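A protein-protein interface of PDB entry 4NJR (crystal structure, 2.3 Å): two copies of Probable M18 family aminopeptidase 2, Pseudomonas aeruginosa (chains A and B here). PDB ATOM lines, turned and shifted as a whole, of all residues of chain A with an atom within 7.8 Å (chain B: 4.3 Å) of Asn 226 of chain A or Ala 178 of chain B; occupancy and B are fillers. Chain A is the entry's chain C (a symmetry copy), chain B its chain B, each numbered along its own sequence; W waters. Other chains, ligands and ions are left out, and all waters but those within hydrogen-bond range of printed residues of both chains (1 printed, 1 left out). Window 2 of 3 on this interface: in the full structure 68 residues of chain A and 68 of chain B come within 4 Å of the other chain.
The backbone NH (N) of Leu 225 of chain A lies within hydrogen-bond range of the backbone carbonyl oxygen (O) of Ile 177 of chain B (2.9 Å).
N of Gln 179 of chain B lies within hydrogen-bond range of OE2 of Glu 228 of chain A.
The side-chain amide oxygen of Gln 179 of chain B sits at hydrogen-bond distance from the side-chain amide nitrogen of Asn 329 of chain A (2.9 Å).
The backbone carbonyl oxygen (O) of Val 223 of chain A lies within hydrogen-bond range of the backbone NH (N) of Glu 228 of chain A (3.4 Å).
O of Phe 229 of chain A sits at hydrogen-bond distance from N of Val 223 of chain A (2.9 Å).
The backbone NH (N) of Asn 226 of chain A lies within hydrogen-bond range of the side-chain carboxylate (OE1) of Glu 228 of chain A (2.8 Å).
N of Ser 409 of chain A lies within hydrogen-bond range of O of Glu 228 of chain A.
The side-chain amide oxygen (OD1) of Asn 329 of chain A sits at hydrogen-bond distance from the backbone NH (N) of Ser 409 of chain A (3.2 Å).
N of His 410 of chain A sits at hydrogen-bond distance from OD1 of Asn 329 of chain A (2.7 Å).
C of Gly 224 of chain A touches O of Ile 177 of chain B (3.9 Å).
Asn 226 of chain A touches Ala 178 of chain B (ND2 to CB, 3.8 Å).
O of Ile 177 of chain B touches OE1 of Glu 228 of chain A, 3.7 Å away.
Glu 228 of chain A touches Ala 178 of chain B.
Phe 229 of chain A touches Phe 101 of chain B (CE1 to CE1, 3.9 Å).
Phe 229 of chain A touches Ile 176 of chain B (CZ to CG2, 3.6 Å).
CD2 of Phe 101 of chain B touches CG of Pro 314 of chain A, 3.7 Å away.
CD1 of Ile 176 of chain B touches CG of Pro 314 of chain A, 3.8 Å away.
Of the printed residues of chain B, Asn 226 of chain A touches Ala 178.
Of the printed residues of chain B, Pro 314 of chain A touches Phe 101 and Ile 176.
Leu 102 of chain B touches none of the printed residues of chain A.
Of the printed residues of chain A, Ile 177 of chain B touches Gly 224 (3.9 Å), Leu 225 (2.9 Å) and Glu 228 (3.7 Å).
The nearest printed residue of chain B that does not touch Asn 226 of chain A is Ile 177 of chain B (4.6 Å).
The nearest residue of chain A that does not touch Ala 178 of chain B is Leu 225 of chain A (4.1 Å).
The nearest printed residue of chain B that does not touch Pro 314 of chain A is Leu 102 of chain B (7.1 Å).
Of the 12 printed residues of chain A, 7 touch a printed residue of chain B.
Hydrophobic or aromatic side chains of chain A within 4 Å of the printed part of chain B: Leu 225, Phe 229 and Pro 314.
Along chain A the printed residues that touch a printed residue of chain B span positions 224 to 329.
Of the 6 printed residues of chain B, 5 touch a printed residue of chain A.
Hydrophobic or aromatic side chains of chain B that line the printed part of chain A: Phe 101, Ile 176 and Ala 178.
Among the printed residues, 11 pairs touch across the chains.
Among the printed residues, no Asp or Glu carboxylate lies within 4 Å of a Lys or Arg side-chain nitrogen of the other chain.
No position is printed for both chains.
Of the 11 pairs that touch across the chains among the printed residues, none has its exchanged pair printed and touching as well.
Water W1 lies within hydrogen-bond range of the side-chain carboxylate (OE2) of Glu 228 of chain A (2.5 Å) and the backbone carbonyl oxygen (O) of Gln 179 of chain B (3.1 Å).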
ATOM      1  N   VAL A 222      -4.553 -13.786  -1.677  1.00  0.00           N
ATOM      2  CA  VAL A 222      -3.656 -14.836  -2.110  1.00  0.00           C
ATOM      3  C   VAL A 222      -4.104 -15.190  -3.525  1.00  0.00           C
ATOM      4  O   VAL A 222      -5.254 -15.065  -3.830  1.00  0.00           O
ATOM      5  CB  VAL A 222      -3.759 -15.984  -1.140  1.00  0.00           C
ATOM      6  CG1 VAL A 222      -2.822 -17.114  -1.497  1.00  0.00           C
ATOM      7  CG2 VAL A 222      -3.444 -15.454   0.244  1.00  0.00           C
ATOM      8  N   VAL A 223      -3.180 -15.452  -4.429  1.00  0.00           N
ATOM      9  CA  VAL A 223      -3.496 -15.743  -5.824  1.00  0.00           C
ATOM     10  C   VAL A 223      -2.544 -16.846  -6.300  1.00  0.00           C
ATOM     11  O   VAL A 223      -1.411 -17.037  -5.758  1.00  0.00           O
ATOM     12  CB  VAL A 223      -3.390 -14.506  -6.757  1.00  0.00           C
ATOM     13  CG1 VAL A 223      -4.232 -13.358  -6.298  1.00  0.00           C
ATOM     14  CG2 VAL A 223      -2.013 -14.004  -6.854  1.00  0.00           C
ATOM     15  N   GLY A 224      -2.984 -17.609  -7.289  1.00  0.00           N
ATOM     16  CA  GLY A 224      -2.162 -18.643  -7.818  1.00  0.00           C
ATOM     17  C   GLY A 224      -2.744 -20.036  -7.662  1.00  0.00           C
ATOM     18  O   GLY A 224      -3.464 -20.329  -6.725  1.00  0.00           O
ATOM     19  N   LEU A 225      -2.407 -20.892  -8.618  1.00  0.00           N
ATOM     20  CA  LEU A 225      -2.880 -22.242  -8.621  1.00  0.00           C
ATOM     21  C   LEU A 225      -2.612 -22.926  -7.279  1.00  0.00           C
ATOM     22  O   LEU A 225      -3.439 -23.629  -6.777  1.00  0.00           O
ATOM     23  CB  LEU A 225      -2.207 -23.010  -9.743  1.00  0.00           C
ATOM     24  CG  LEU A 225      -2.761 -24.432  -9.848  1.00  0.00           C
ATOM     25  CD1 LEU A 225      -4.251 -24.394 -10.197  1.00  0.00           C
ATOM     26  CD2 LEU A 225      -1.957 -25.241 -10.855  1.00  0.00           C
ATOM     27  N   ASN A 226      -1.442 -22.727  -6.727  1.00  0.00           N
ATOM     28  CA  ASN A 226      -1.102 -23.299  -5.439  1.00  0.00           C
ATOM     29  C   ASN A 226      -0.886 -22.212  -4.372  1.00  0.00           C
ATOM     30  O   ASN A 226      -0.097 -22.425  -3.459  1.00  0.00           O
ATOM     31  CB  ASN A 226       0.148 -24.159  -5.548  1.00  0.00           C
ATOM     32  CG  ASN A 226       0.064 -25.124  -6.711  1.00  0.00           C
ATOM     33  OD1 ASN A 226      -0.720 -26.046  -6.679  1.00  0.00           O
ATOM     34  ND2 ASN A 226       0.816 -24.877  -7.760  1.00  0.00           N
ATOM     35  N   ASP A 227      -1.595 -21.076  -4.500  1.00  0.00           N
ATOM     36  CA  ASP A 227      -1.501 -19.980  -3.526  1.00  0.00           C
ATOM     37  C   ASP A 227      -0.093 -19.492  -3.343  1.00  0.00           C
ATOM     38  O   ASP A 227       0.355 -19.204  -2.208  1.00  0.00           O
ATOM     39  CB  ASP A 227      -2.082 -20.432  -2.171  1.00  0.00           C
ATOM     40  CG  ASP A 227      -3.553 -20.832  -2.262  1.00  0.00           C
ATOM     41  OD1 ASP A 227      -4.329 -20.475  -3.190  1.00  0.00           O
ATOM     42  OD2 ASP A 227      -3.949 -21.556  -1.386  1.00  0.00           O
ATOM     43  N   GLU A 228       0.631 -19.408  -4.457  1.00  0.00           N
ATOM     44  CA  GLU A 228       2.017 -19.025  -4.412  1.00  0.00           C
ATOM     45  C   GLU A 228       2.259 -17.564  -4.103  1.00  0.00           C
ATOM     46  O   GLU A 228       3.362 -17.175  -3.713  1.00  0.00           O
ATOM     47  CB  GLU A 228       2.651 -19.333  -5.766  1.00  0.00           C
ATOM     48  CG  GLU A 228       2.853 -20.812  -6.031  1.00  0.00           C
ATOM     49  CD  GLU A 228       1.806 -21.363  -6.968  1.00  0.00           C
ATOM     50  OE1 GLU A 228       0.601 -20.850  -7.074  1.00  0.00           O
ATOM     51  OE2 GLU A 228       2.237 -22.344  -7.591  1.00  0.00           O
ATOM     52  N   PHE A 229       1.267 -16.751  -4.392  1.00  0.00           N
ATOM     53  CA  PHE A 229       1.446 -15.328  -4.450  1.00  0.00           C
ATOM     54  C   PHE A 229       0.493 -14.513  -3.591  1.00  0.00           C
ATOM     55  O   PHE A 229      -0.628 -14.952  -3.230  1.00  0.00           O
ATOM     56  CB  PHE A 229       1.287 -14.854  -5.891  1.00  0.00           C
ATOM     57  CG  PHE A 229       2.025 -15.694  -6.924  1.00  0.00           C
ATOM     58  CD1 PHE A 229       3.383 -15.761  -6.935  1.00  0.00           C
ATOM     59  CD2 PHE A 229       1.315 -16.400  -7.910  1.00  0.00           C
ATOM     60  CE1 PHE A 229       4.065 -16.549  -7.861  1.00  0.00           C
ATOM     61  CE2 PHE A 229       2.002 -17.159  -8.886  1.00  0.00           C
ATOM     62  CZ  PHE A 229       3.387 -17.245  -8.847  1.00  0.00           C
ATOM     63  N   PRO A 314       9.204 -13.312 -15.764  1.00  0.00           N
ATOM     64  CA  PRO A 314       9.432 -14.155 -16.930  1.00  0.00           C
ATOM     65  C   PRO A 314       8.977 -13.581 -18.246  1.00  0.00           C
ATOM     66  O   PRO A 314       9.348 -14.115 -19.259  1.00  0.00           O
ATOM     67  CB  PRO A 314       8.603 -15.416 -16.619  1.00  0.00           C
ATOM     68  CG  PRO A 314       7.501 -14.918 -15.687  1.00  0.00           C
ATOM     69  CD  PRO A 314       8.169 -13.849 -14.855  1.00  0.00           C
ATOM     70  N   ASN A 329       9.270 -16.311  -3.451  1.00  0.00           N
ATOM     71  CA  ASN A 329       9.267 -17.492  -2.579  1.00  0.00           C
ATOM     72  C   ASN A 329      10.614 -18.136  -2.409  1.00  0.00           C
ATOM     73  O   ASN A 329      10.722 -19.237  -1.887  1.00  0.00           O
ATOM     74  CB  ASN A 329       8.206 -18.511  -3.008  1.00  0.00           C
ATOM     75  CG  ASN A 329       6.823 -17.979  -2.827  1.00  0.00           C
ATOM     76  OD1 ASN A 329       6.512 -17.388  -1.777  1.00  0.00           O
ATOM     77  ND2 ASN A 329       5.995 -18.102  -3.867  1.00  0.00           N
ATOM     78  N   SER A 409       3.831 -15.633  -1.424  1.00  0.00           N
ATOM     79  CA  SER A 409       3.107 -15.922  -0.191  1.00  0.00           C
ATOM     80  C   SER A 409       3.959 -16.644   0.865  1.00  0.00           C
ATOM     81  O   SER A 409       3.500 -16.811   1.958  1.00  0.00           O
ATOM     82  CB  SER A 409       1.866 -16.768  -0.506  1.00  0.00           C
ATOM     83  OG  SER A 409       2.277 -18.038  -0.985  1.00  0.00           O
ATOM     84  N   HIS A 410       5.154 -17.122   0.539  1.00  0.00           N
ATOM     85  CA  HIS A 410       6.014 -17.794   1.509  1.00  0.00           C
ATOM     86  C   HIS A 410       7.009 -16.809   2.111  1.00  0.00           C
ATOM     87  O   HIS A 410       7.668 -17.113   3.083  1.00  0.00           O
ATOM     88  CB  HIS A 410       6.826 -18.899   0.818  1.00  0.00           C
ATOM     89  CG  HIS A 410       5.988 -20.048   0.343  1.00  0.00           C
ATOM     90  ND1 HIS A 410       6.366 -21.358   0.483  1.00  0.00           N
ATOM     91  CD2 HIS A 410       4.756 -20.084  -0.205  1.00  0.00           C
ATOM     92  CE1 HIS A 410       5.407 -22.149   0.055  1.00  0.00           C
ATOM     93  NE2 HIS A 410       4.424 -21.399  -0.384  1.00  0.00           N
ATOM     94  N   PHE B 101       8.675 -20.399 -13.187  1.00  0.00           N
ATOM     95  CA  PHE B 101       7.196 -20.304 -13.281  1.00  0.00           C
ATOM     96  C   PHE B 101       6.580 -21.234 -14.340  1.00  0.00           C
ATOM     97  O   PHE B 101       7.196 -21.564 -15.348  1.00  0.00           O
ATOM     98  CB  PHE B 101       6.744 -18.898 -13.616  1.00  0.00           C
ATOM     99  CG  PHE B 101       7.185 -17.876 -12.642  1.00  0.00           C
ATOM    100  CD1 PHE B 101       6.490 -17.705 -11.442  1.00  0.00           C
ATOM    101  CD2 PHE B 101       8.351 -17.152 -12.863  1.00  0.00           C
ATOM    102  CE1 PHE B 101       6.880 -16.746 -10.568  1.00  0.00           C
ATOM    103  CE2 PHE B 101       8.781 -16.212 -11.957  1.00  0.00           C
ATOM    104  CZ  PHE B 101       8.042 -15.998 -10.818  1.00  0.00           C
ATOM    105  N   LEU B 102       5.323 -21.536 -14.140  1.00  0.00           N
ATOM    106  CA  LEU B 102       4.458 -22.026 -15.191  1.00  0.00           C
ATOM    107  C   LEU B 102       3.514 -20.883 -15.585  1.00  0.00           C
ATOM    108  O   LEU B 102       2.772 -20.320 -14.752  1.00  0.00           O
ATOM    109  CB  LEU B 102       3.630 -23.228 -14.700  1.00  0.00           C
ATOM    110  CG  LEU B 102       2.610 -23.766 -15.677  1.00  0.00           C
ATOM    111  CD1 LEU B 102       3.256 -24.244 -16.946  1.00  0.00           C
ATOM    112  CD2 LEU B 102       1.849 -24.917 -15.091  1.00  0.00           C
ATOM    113  N   ILE B 176       1.049 -15.807 -15.433  1.00  0.00           N
ATOM    114  CA  ILE B 176       1.612 -16.739 -14.429  1.00  0.00           C
ATOM    115  C   ILE B 176       0.485 -17.350 -13.634  1.00  0.00           C
ATOM    116  O   ILE B 176      -0.396 -16.657 -13.139  1.00  0.00           O
ATOM    117  CB  ILE B 176       2.550 -15.996 -13.436  1.00  0.00           C
ATOM    118  CG1 ILE B 176       3.652 -15.284 -14.220  1.00  0.00           C
ATOM    119  CG2 ILE B 176       3.232 -16.948 -12.455  1.00  0.00           C
ATOM    120  CD1 ILE B 176       4.512 -14.381 -13.354  1.00  0.00           C
ATOM    121  N   ILE B 177       0.507 -18.665 -13.571  1.00  0.00           N
ATOM    122  CA  ILE B 177      -0.434 -19.483 -12.778  1.00  0.00           C
ATOM    123  C   ILE B 177       0.246 -20.294 -11.650  1.00  0.00           C
ATOM    124  O   ILE B 177      -0.401 -20.655 -10.661  1.00  0.00           O
ATOM    125  CB  ILE B 177      -1.269 -20.460 -13.631  1.00  0.00           C
ATOM    126  CG1 ILE B 177      -0.427 -21.637 -14.115  1.00  0.00           C
ATOM    127  CG2 ILE B 177      -1.952 -19.792 -14.837  1.00  0.00           C
ATOM    128  CD1 ILE B 177      -1.317 -22.721 -14.700  1.00  0.00           C
ATOM    129  N   ALA B 178       1.542 -20.551 -11.757  1.00  0.00           N
ATOM    130  CA  ALA B 178       2.192 -21.314 -10.727  1.00  0.00           C
ATOM    131  C   ALA B 178       3.740 -21.218 -10.767  1.00  0.00           C
ATOM    132  O   ALA B 178       4.326 -20.626 -11.649  1.00  0.00           O
ATOM    133  CB  ALA B 178       1.742 -22.786 -10.804  1.00  0.00           C
ATOM    134  N   GLN B 179       4.361 -21.826  -9.764  1.00  0.00           N
ATOM    135  CA  GLN B 179       5.779 -22.088  -9.764  1.00  0.00           C
ATOM    136  C   GLN B 179       5.963 -23.601  -9.860  1.00  0.00           C
ATOM    137  O   GLN B 179       5.132 -24.359  -9.407  1.00  0.00           O
ATOM    138  CB  GLN B 179       6.365 -21.524  -8.489  1.00  0.00           C
ATOM    139  CG  GLN B 179       6.539 -20.039  -8.595  1.00  0.00           C
ATOM    140  CD  GLN B 179       7.052 -19.425  -7.349  1.00  0.00           C
ATOM    141  OE1 GLN B 179       6.509 -19.625  -6.283  1.00  0.00           O
ATOM    142  NE2 GLN B 179       8.108 -18.650  -7.469  1.00  0.00           N
HETATM  143  O   HOH W   1       3.965 -23.800  -6.617  1.00  0.00           O
